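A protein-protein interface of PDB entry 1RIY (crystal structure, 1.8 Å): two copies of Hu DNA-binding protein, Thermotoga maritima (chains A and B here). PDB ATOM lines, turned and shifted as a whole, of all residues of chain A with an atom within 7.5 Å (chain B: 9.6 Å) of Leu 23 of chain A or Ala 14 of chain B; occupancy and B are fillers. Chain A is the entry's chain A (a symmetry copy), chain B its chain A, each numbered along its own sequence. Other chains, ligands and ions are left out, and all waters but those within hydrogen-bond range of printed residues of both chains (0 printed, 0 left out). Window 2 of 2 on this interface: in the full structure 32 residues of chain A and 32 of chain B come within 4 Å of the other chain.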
ATOM      1  N   ILE A   7     -36.799  21.743  -9.436  1.00  0.00           N
ATOM      2  CA  ILE A   7     -35.489  22.400  -9.245  1.00  0.00           C
ATOM      3  C   ILE A   7     -35.679  23.748  -8.551  1.00  0.00           C
ATOM      4  O   ILE A   7     -34.971  24.065  -7.607  1.00  0.00           O
ATOM      5  CB  ILE A   7     -34.760  22.568 -10.606  1.00  0.00           C
ATOM      6  CG1 ILE A   7     -34.218  21.231 -11.089  1.00  0.00           C
ATOM      7  CG2 ILE A   7     -33.611  23.575 -10.537  1.00  0.00           C
ATOM      8  CD1 ILE A   7     -33.933  21.221 -12.540  1.00  0.00           C
ATOM      9  N   LYS A  17     -28.144  27.704  -5.608  1.00  0.00           N
ATOM     10  CA  LYS A  17     -28.306  28.265  -6.937  1.00  0.00           C
ATOM     11  C   LYS A  17     -29.041  27.215  -7.794  1.00  0.00           C
ATOM     12  O   LYS A  17     -28.774  26.016  -7.674  1.00  0.00           O
ATOM     13  CB  LYS A  17     -26.945  28.511  -7.536  1.00  0.00           C
ATOM     14  CG  LYS A  17     -26.085  29.536  -6.766  1.00  0.00           C
ATOM     15  CD  LYS A  17     -24.816  29.846  -7.513  1.00  0.00           C
ATOM     16  CE  LYS A  17     -23.928  30.807  -6.724  1.00  0.00           C
ATOM     17  NZ  LYS A  17     -22.522  30.910  -7.232  1.00  0.00           N
ATOM     18  N   LYS A  18     -29.933  27.674  -8.665  1.00  0.00           N
ATOM     19  CA  LYS A  18     -30.649  26.749  -9.545  1.00  0.00           C
ATOM     20  C   LYS A  18     -29.706  25.863 -10.360  1.00  0.00           C
ATOM     21  O   LYS A  18     -29.973  24.669 -10.520  1.00  0.00           O
ATOM     22  CB  LYS A  18     -31.589  27.514 -10.473  1.00  0.00           C
ATOM     23  CG  LYS A  18     -32.792  28.079  -9.776  1.00  0.00           C
ATOM     24  CD  LYS A  18     -33.598  29.002 -10.720  1.00  0.00           C
ATOM     25  CE  LYS A  18     -34.745  29.726 -10.016  1.00  0.00           C
ATOM     26  NZ  LYS A  18     -35.706  30.385 -11.030  1.00  0.00           N
ATOM     27  N   LYS A  19     -28.602  26.420 -10.863  1.00  0.00           N
ATOM     28  CA  LYS A  19     -27.687  25.622 -11.641  1.00  0.00           C
ATOM     29  C   LYS A  19     -27.100  24.477 -10.835  1.00  0.00           C
ATOM     30  O   LYS A  19     -26.857  23.373 -11.376  1.00  0.00           O
ATOM     31  CB  LYS A  19     -26.583  26.461 -12.273  1.00  0.00           C
ATOM     32  CG  LYS A  19     -25.480  26.939 -11.341  1.00  0.00           C
ATOM     33  CD  LYS A  19     -24.443  27.705 -12.138  1.00  0.00           C
ATOM     34  CE  LYS A  19     -23.650  28.657 -11.252  1.00  0.00           C
ATOM     35  N   ASP A  20     -26.877  24.707  -9.545  1.00  0.00           N
ATOM     36  CA  ASP A  20     -26.303  23.668  -8.687  1.00  0.00           C
ATOM     37  C   ASP A  20     -27.351  22.584  -8.334  1.00  0.00           C
ATOM     38  O   ASP A  20     -27.016  21.406  -8.297  1.00  0.00           O
ATOM     39  CB  ASP A  20     -25.720  24.258  -7.423  1.00  0.00           C
ATOM     40  CG  ASP A  20     -24.488  25.106  -7.698  1.00  0.00           C
ATOM     41  OD1 ASP A  20     -23.797  24.856  -8.720  1.00  0.00           O
ATOM     42  OD2 ASP A  20     -24.130  26.040  -6.935  1.00  0.00           O
ATOM     43  N   VAL A  21     -28.603  22.997  -8.103  1.00  0.00           N
ATOM     44  CA  VAL A  21     -29.684  22.045  -7.866  1.00  0.00           C
ATOM     45  C   VAL A  21     -29.871  21.211  -9.133  1.00  0.00           C
ATOM     46  O   VAL A  21     -30.013  19.972  -9.081  1.00  0.00           O
ATOM     47  CB  VAL A  21     -30.979  22.739  -7.435  1.00  0.00           C
ATOM     48  CG1 VAL A  21     -32.126  21.745  -7.298  1.00  0.00           C
ATOM     49  CG2 VAL A  21     -30.768  23.472  -6.111  1.00  0.00           C
ATOM     50  N   LYS A  22     -29.880  21.875 -10.292  1.00  0.00           N
ATOM     51  CA  LYS A  22     -30.005  21.101 -11.548  1.00  0.00           C
ATOM     52  C   LYS A  22     -28.901  20.050 -11.716  1.00  0.00           C
ATOM     53  O   LYS A  22     -29.175  18.920 -12.079  1.00  0.00           O
ATOM     54  CB  LYS A  22     -30.015  22.029 -12.753  1.00  0.00           C
ATOM     55  CG  LYS A  22     -30.140  21.272 -14.033  1.00  0.00           C
ATOM     56  CD  LYS A  22     -30.446  22.175 -15.264  1.00  0.00           C
ATOM     57  N   LEU A  23     -27.645  20.431 -11.441  1.00  0.00           N
ATOM     58  CA  LEU A  23     -26.513  19.529 -11.554  1.00  0.00           C
ATOM     59  C   LEU A  23     -26.671  18.350 -10.635  1.00  0.00           C
ATOM     60  O   LEU A  23     -26.548  17.200 -11.056  1.00  0.00           O
ATOM     61  CB  LEU A  23     -25.191  20.229 -11.166  1.00  0.00           C
ATOM     62  CG  LEU A  23     -23.930  19.330 -11.042  1.00  0.00           C
ATOM     63  CD1 LEU A  23     -23.624  18.581 -12.331  1.00  0.00           C
ATOM     64  CD2 LEU A  23     -22.666  20.099 -10.627  1.00  0.00           C
ATOM     65  N   ILE A  24     -26.971  18.650  -9.396  1.00  0.00           N
ATOM     66  CA  ILE A  24     -27.052  17.594  -8.377  1.00  0.00           C
ATOM     67  C   ILE A  24     -28.266  16.680  -8.618  1.00  0.00           C
ATOM     68  O   ILE A  24     -28.134  15.456  -8.572  1.00  0.00           O
ATOM     69  CB  ILE A  24     -26.995  18.185  -6.989  1.00  0.00           C
ATOM     70  CG1 ILE A  24     -25.584  18.695  -6.713  1.00  0.00           C
ATOM     71  CG2 ILE A  24     -27.350  17.111  -5.960  1.00  0.00           C
ATOM     72  CD1 ILE A  24     -25.524  19.598  -5.492  1.00  0.00           C
ATOM     73  N   LEU A  25     -29.416  17.258  -8.927  1.00  0.00           N
ATOM     74  CA  LEU A  25     -30.582  16.440  -9.263  1.00  0.00           C
ATOM     75  C   LEU A  25     -30.277  15.559 -10.461  1.00  0.00           C
ATOM     76  O   LEU A  25     -30.572  14.347 -10.479  1.00  0.00           O
ATOM     77  CB  LEU A  25     -31.794  17.323  -9.584  1.00  0.00           C
ATOM     78  CG  LEU A  25     -33.004  16.588 -10.136  1.00  0.00           C
ATOM     79  CD1 LEU A  25     -33.576  15.558  -9.151  1.00  0.00           C
ATOM     80  CD2 LEU A  25     -34.111  17.558 -10.525  1.00  0.00           C
ATOM     81  N   ASP A  26     -29.736  16.158 -11.521  1.00  0.00           N
ATOM     82  CA  ASP A  26     -29.424  15.378 -12.737  1.00  0.00           C
ATOM     83  C   ASP A  26     -28.417  14.249 -12.476  1.00  0.00           C
ATOM     84  O   ASP A  26     -28.489  13.156 -13.070  1.00  0.00           O
ATOM     85  CB  ASP A  26     -28.893  16.285 -13.850  1.00  0.00           C
ATOM     86  CG  ASP A  26     -30.002  17.060 -14.508  1.00  0.00           C
ATOM     87  OD1 ASP A  26     -31.161  16.773 -14.247  1.00  0.00           O
ATOM     88  OD2 ASP A  26     -29.786  17.973 -15.332  1.00  0.00           O
ATOM     89  N   THR A  27     -27.462  14.523 -11.610  1.00  0.00           N
ATOM     90  CA  THR A  27     -26.463  13.519 -11.243  1.00  0.00           C
ATOM     91  C   THR A  27     -27.123  12.403 -10.385  1.00  0.00           C
ATOM     92  O   THR A  27     -26.768  11.230 -10.507  1.00  0.00           O
ATOM     93  CB  THR A  27     -25.301  14.187 -10.527  1.00  0.00           C
ATOM     94  OG1 THR A  27     -24.724  15.226 -11.385  1.00  0.00           O
ATOM     95  CG2 THR A  27     -24.177  13.229 -10.318  1.00  0.00           C
ATOM     96  N   ILE A  28     -28.028  12.767  -9.517  1.00  0.00           N
ATOM     97  CA  ILE A  28     -28.769  11.763  -8.734  1.00  0.00           C
ATOM     98  C   ILE A  28     -29.550  10.866  -9.670  1.00  0.00           C
ATOM     99  O   ILE A  28     -29.502   9.646  -9.585  1.00  0.00           O
ATOM    100  CB  ILE A  28     -29.765  12.470  -7.754  1.00  0.00           C
ATOM    101  CG1 ILE A  28     -29.039  13.102  -6.570  1.00  0.00           C
ATOM    102  CG2 ILE A  28     -30.731  11.477  -7.211  1.00  0.00           C
ATOM    103  CD1 ILE A  28     -29.830  14.214  -5.923  1.00  0.00           C
ATOM    104  N   LEU A  29     -30.257  11.463 -10.616  1.00  0.00           N
ATOM    105  CA  LEU A  29     -31.060  10.688 -11.560  1.00  0.00           C
ATOM    106  C   LEU A  29     -30.193   9.770 -12.420  1.00  0.00           C
ATOM    107  O   LEU A  29     -30.555   8.620 -12.676  1.00  0.00           O
ATOM    108  CB  LEU A  29     -31.884  11.617 -12.446  1.00  0.00           C
ATOM    109  CG  LEU A  29     -32.893  12.488 -11.680  1.00  0.00           C
ATOM    110  CD1 LEU A  29     -33.602  13.347 -12.702  1.00  0.00           C
ATOM    111  CD2 LEU A  29     -33.888  11.685 -10.912  1.00  0.00           C
ATOM    112  N   LEU B   6     -25.314   6.695  -2.219  1.00  0.00           N
ATOM    113  CA  LEU B   6     -25.873   7.568  -3.271  1.00  0.00           C
ATOM    114  C   LEU B   6     -25.299   8.970  -3.132  1.00  0.00           C
ATOM    115  O   LEU B   6     -24.837   9.574  -4.102  1.00  0.00           O
ATOM    116  CB  LEU B   6     -27.393   7.601  -3.177  1.00  0.00           C
ATOM    117  CG  LEU B   6     -28.138   8.560  -4.086  1.00  0.00           C
ATOM    118  CD1 LEU B   6     -27.857   8.236  -5.568  1.00  0.00           C
ATOM    119  CD2 LEU B   6     -29.650   8.552  -3.830  1.00  0.00           C
ATOM    120  N   ILE B   7     -25.329   9.514  -1.926  1.00  0.00           N
ATOM    121  CA  ILE B   7     -24.781  10.865  -1.684  1.00  0.00           C
ATOM    122  C   ILE B   7     -23.305  10.907  -2.079  1.00  0.00           C
ATOM    123  O   ILE B   7     -22.870  11.825  -2.756  1.00  0.00           O
ATOM    124  CB  ILE B   7     -24.976  11.274  -0.199  1.00  0.00           C
ATOM    125  CG1 ILE B   7     -26.432  11.623   0.071  1.00  0.00           C
ATOM    126  CG2 ILE B   7     -24.098  12.459   0.205  1.00  0.00           C
ATOM    127  CD1 ILE B   7     -26.775  11.570   1.509  1.00  0.00           C
ATOM    128  N   ASP B   8     -22.527   9.923  -1.629  1.00  0.00           N
ATOM    129  CA  ASP B   8     -21.091   9.852  -1.928  1.00  0.00           C
ATOM    130  C   ASP B   8     -20.761   9.772  -3.425  1.00  0.00           C
ATOM    131  O   ASP B   8     -19.861  10.489  -3.919  1.00  0.00           O
ATOM    132  CB  ASP B   8     -20.446   8.651  -1.214  1.00  0.00           C
ATOM    133  CG  ASP B   8     -20.405   8.821   0.316  1.00  0.00           C
ATOM    134  OD1 ASP B   8     -20.720   9.925   0.830  1.00  0.00           O
ATOM    135  OD2 ASP B   8     -20.087   7.871   1.071  1.00  0.00           O
ATOM    136  N   ARG B   9     -21.472   8.916  -4.159  1.00  0.00           N
ATOM    137  CA  ARG B   9     -21.244   8.772  -5.593  1.00  0.00           C
ATOM    138  C   ARG B   9     -21.633  10.036  -6.329  1.00  0.00           C
ATOM    139  O   ARG B   9     -20.943  10.442  -7.270  1.00  0.00           O
ATOM    140  CB  ARG B   9     -22.064   7.634  -6.191  1.00  0.00           C
ATOM    141  CG  ARG B   9     -21.547   6.210  -5.836  1.00  0.00           C
ATOM    142  CD  ARG B   9     -22.565   5.098  -6.123  1.00  0.00           C
ATOM    143  NE  ARG B   9     -22.313   3.813  -5.435  1.00  0.00           N
ATOM    144  CZ  ARG B   9     -21.533   3.625  -4.370  1.00  0.00           C
ATOM    145  NH1 ARG B   9     -20.864   4.631  -3.779  1.00  0.00           N
ATOM    146  NH2 ARG B   9     -21.442   2.402  -3.866  1.00  0.00           N
ATOM    147  N   VAL B  10     -22.753  10.645  -5.936  1.00  0.00           N
ATOM    148  CA  VAL B  10     -23.165  11.891  -6.568  1.00  0.00           C
ATOM    149  C   VAL B  10     -22.194  13.036  -6.256  1.00  0.00           C
ATOM    150  O   VAL B  10     -21.798  13.788  -7.139  1.00  0.00           O
ATOM    151  CB  VAL B  10     -24.611  12.275  -6.109  1.00  0.00           C
ATOM    152  CG1 VAL B  10     -24.928  13.703  -6.533  1.00  0.00           C
ATOM    153  CG2 VAL B  10     -25.585  11.288  -6.686  1.00  0.00           C
ATOM    154  N   ALA B  11     -21.762  13.118  -5.005  1.00  0.00           N
ATOM    155  CA  ALA B  11     -20.827  14.161  -4.622  1.00  0.00           C
ATOM    156  C   ALA B  11     -19.529  14.051  -5.476  1.00  0.00           C
ATOM    157  O   ALA B  11     -19.001  15.049  -5.942  1.00  0.00           O
ATOM    158  CB  ALA B  11     -20.481  14.061  -3.183  1.00  0.00           C
ATOM    159  N   LYS B  12     -19.046  12.825  -5.661  1.00  0.00           N
ATOM    160  CA  LYS B  12     -17.840  12.612  -6.464  1.00  0.00           C
ATOM    161  C   LYS B  12     -18.048  13.027  -7.920  1.00  0.00           C
ATOM    162  O   LYS B  12     -17.221  13.733  -8.506  1.00  0.00           O
ATOM    163  CB  LYS B  12     -17.424  11.144  -6.427  1.00  0.00           C
ATOM    164  CG  LYS B  12     -16.228  10.830  -7.277  1.00  0.00           C
ATOM    165  CD  LYS B  12     -15.852   9.322  -7.183  1.00  0.00           C
ATOM    166  CE  LYS B  12     -14.894   8.892  -8.326  1.00  0.00           C
ATOM    167  NZ  LYS B  12     -14.644   7.397  -8.322  1.00  0.00           N
ATOM    168  N   LYS B  13     -19.144  12.582  -8.501  1.00  0.00           N
ATOM    169  CA  LYS B  13     -19.415  12.834  -9.914  1.00  0.00           C
ATOM    170  C   LYS B  13     -19.671  14.290 -10.194  1.00  0.00           C
ATOM    171  O   LYS B  13     -19.208  14.807 -11.220  1.00  0.00           O
ATOM    172  CB  LYS B  13     -20.598  12.034 -10.418  1.00  0.00           C
ATOM    173  CG  LYS B  13     -20.346  10.539 -10.478  1.00  0.00           C
ATOM    174  CD  LYS B  13     -21.544   9.873 -11.151  1.00  0.00           C
ATOM    175  CE  LYS B  13     -21.721   8.429 -10.708  1.00  0.00           C
ATOM    176  NZ  LYS B  13     -22.973   7.842 -11.270  1.00  0.00           N
ATOM    177  N   ALA B  14     -20.388  14.956  -9.294  1.00  0.00           N
ATOM    178  CA  ALA B  14     -20.722  16.363  -9.465  1.00  0.00           C
ATOM    179  C   ALA B  14     -19.633  17.319  -8.971  1.00  0.00           C
ATOM    180  O   ALA B  14     -19.751  18.530  -9.188  1.00  0.00           O
ATOM    181  CB  ALA B  14     -22.012  16.681  -8.748  1.00  0.00           C
ATOM    182  N   GLY B  15     -18.643  16.804  -8.254  1.00  0.00           N
ATOM    183  CA  GLY B  15     -17.609  17.656  -7.655  1.00  0.00           C
ATOM    184  C   GLY B  15     -18.157  18.576  -6.570  1.00  0.00           C
ATOM    185  O   GLY B  15     -17.769  19.726  -6.428  1.00  0.00           O
ATOM    186  N   ALA B  16     -19.098  18.053  -5.803  1.00  0.00           N
ATOM    187  CA  ALA B  16     -19.779  18.802  -4.771  1.00  0.00           C
ATOM    188  C   ALA B  16     -19.463  18.246  -3.403  1.00  0.00           C
ATOM    189  O   ALA B  16     -19.101  17.070  -3.240  1.00  0.00           O
ATOM    190  CB  ALA B  16     -21.259  18.765  -5.015  1.00  0.00           C
ATOM    191  N   LYS B  17     -19.597  19.106  -2.401  1.00  0.00           N
ATOM    192  CA  LYS B  17     -19.314  18.676  -1.043  1.00  0.00           C
ATOM    193  C   LYS B  17     -20.440  17.713  -0.621  1.00  0.00           C
ATOM    194  O   LYS B  17     -21.609  17.938  -0.951  1.00  0.00           O
ATOM    195  CB  LYS B  17     -19.337  19.877  -0.133  1.00  0.00           C
ATOM    196  CG  LYS B  17     -18.265  20.941  -0.452  1.00  0.00           C
ATOM    197  CD  LYS B  17     -18.247  22.021   0.594  1.00  0.00           C
ATOM    198  CE  LYS B  17     -17.236  23.113   0.248  1.00  0.00           C
ATOM    199  NZ  LYS B  17     -17.383  24.371   1.050  1.00  0.00           N
ATOM    200  N   LYS B  18     -20.088  16.671   0.125  1.00  0.00           N
ATOM    201  CA  LYS B  18     -21.100  15.728   0.602  1.00  0.00           C
ATOM    202  C   LYS B  18     -22.227  16.415   1.374  1.00  0.00           C
ATOM    203  O   LYS B  18     -23.395  16.058   1.200  1.00  0.00           O
ATOM    204  CB  LYS B  18     -20.456  14.643   1.461  1.00  0.00           C
ATOM    205  CG  LYS B  18     -19.640  13.660   0.674  1.00  0.00           C
ATOM    206  CD  LYS B  18     -18.860  12.709   1.612  1.00  0.00           C
ATOM    207  CE  LYS B  18     -17.893  11.791   0.865  1.00  0.00           C
ATOM    208  NZ  LYS B  18     -17.367  10.660   1.778  1.00  0.00           N
ATOM    209  N   ASP B  20     -23.464  19.292   0.930  1.00  0.00           N
ATOM    210  CA  ASP B  20     -24.353  19.991  -0.001  1.00  0.00           C
ATOM    211  C   ASP B  20     -25.228  18.996  -0.803  1.00  0.00           C
ATOM    212  O   ASP B  20     -26.399  19.270  -1.035  1.00  0.00           O
ATOM    213  CB  ASP B  20     -23.572  20.875  -0.947  1.00  0.00           C
ATOM    214  CG  ASP B  20     -22.929  22.054  -0.235  1.00  0.00           C
ATOM    215  OD1 ASP B  20     -23.455  22.482   0.825  1.00  0.00           O
ATOM    216  OD2 ASP B  20     -21.896  22.624  -0.674  1.00  0.00           O
ATOM    217  N   VAL B  21     -24.653  17.852  -1.191  1.00  0.00           N
ATOM    218  CA  VAL B  21     -25.420  16.806  -1.859  1.00  0.00           C
ATOM    219  C   VAL B  21     -26.478  16.293  -0.882  1.00  0.00           C
ATOM    220  O   VAL B  21     -27.657  16.104  -1.243  1.00  0.00           O
ATOM    221  CB  VAL B  21     -24.524  15.679  -2.384  1.00  0.00           C
ATOM    222  CG1 VAL B  21     -25.347  14.543  -2.979  1.00  0.00           C
ATOM    223  CG2 VAL B  21     -23.555  16.223  -3.432  1.00  0.00           C
ATOM    224  N   ILE B  24     -29.315  18.922  -0.605  1.00  0.00           N
ATOM    225  CA  ILE B  24     -30.120  19.021  -1.830  1.00  0.00           C
ATOM    226  C   ILE B  24     -30.938  17.738  -2.063  1.00  0.00           C
ATOM    227  O   ILE B  24     -32.131  17.814  -2.356  1.00  0.00           O
ATOM    228  CB  ILE B  24     -29.260  19.421  -3.004  1.00  0.00           C
ATOM    229  CG1 ILE B  24     -28.848  20.882  -2.855  1.00  0.00           C
ATOM    230  CG2 ILE B  24     -30.053  19.254  -4.301  1.00  0.00           C
ATOM    231  CD1 ILE B  24     -27.719  21.264  -3.799  1.00  0.00           C
ATOM    232  N   ILE B  28     -34.956  17.565  -2.045  1.00  0.00           N
ATOM    233  CA  ILE B  28     -35.694  16.969  -3.173  1.00  0.00           C
ATOM    234  C   ILE B  28     -36.685  15.952  -2.649  1.00  0.00           C
ATOM    235  O   ILE B  28     -37.858  15.955  -2.997  1.00  0.00           O
ATOM    236  CB  ILE B  28     -34.701  16.260  -4.153  1.00  0.00           C
ATOM    237  CG1 ILE B  28     -33.911  17.267  -4.984  1.00  0.00           C
ATOM    238  CG2 ILE B  28     -35.456  15.392  -5.098  1.00  0.00           C
ATOM    239  CD1 ILE B  28     -32.614  16.701  -5.513  1.00  0.00           C
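The side-chain hydroxyl (OG1) of Thr 27 of chain A lies within hydrogen-bond range of the backbone carbonyl oxygen (O) of Leu 23 of chain A (2.7 Å).
Among the printed residues, merely in contact across the chains: Leu 23 of chain A with Ala 14 of chain B (3.6 Å), Ile 24 of chain A with Ile 24 of chain B (3.2 Å), Leu 25 of chain A with Ile 28 of chain B (3.9 Å), Thr 27 of chain A with Val 10 of chain B (3.9 Å), Thr 27 of chain A with Lys 13 of chain B (3.8 Å), Ile 28 of chain A with Val 10 of chain B (3.8 Å) and Ile 28 of chain A with Ile 28 of chain B (3.8 Å).
Lys 19 of chain A touches none of the printed residues of chain B.
No residue of chain B comes within 4 Å of Lys 22 of chain A.
Of chain B, only Ala 14 (3.6 Å) comes within 4 Å of Leu 23 of chain A.
Of the printed residues of chain B, Thr 27 of chain A touches Val 10 and Lys 13.
Ile 7 of chain B touches none of the printed residues of chain A.
Ala 14 of chain B touches just one residue of chain A: Leu 23.
Of the printed residues of chain A, Ile 28 of chain B touches Leu 25 (3.9 Å) and Ile 28 (3.8 Å).
The nearest residue of chain B that does not touch Leu 23 of chain A is Gly 15 of chain B (5.7 Å).
The nearest printed residue of chain B that does not touch Ile 28 of chain A is Leu 6 of chain B (4.6 Å).
Of the 17 printed residues of chain B, 5 touch a printed residue of chain A.
Printed residues of chain B that touch a printed residue of chain A: Val 10, Lys 13, Ala 14, Ile 24 and Ile 28.
Hydrophobic or aromatic side chains of chain B that line the printed part of chain A: Val 10, Ala 14, Ile 24 and Ile 28.
Hydrophobic or aromatic side chains of chain A that line the printed part of chain B: Leu 23, Ile 24, Leu 25 and Ile 28.
Among the printed residues, no Asp or Glu carboxylate lies within 4 Å of a Lys or Arg side-chain nitrogen of the other chain.
Ile 24 of chain A touches its own counterpart, Ile 24 of chain B.
Ile 28 of chain A touches its own counterpart, Ile 28 of chain B.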
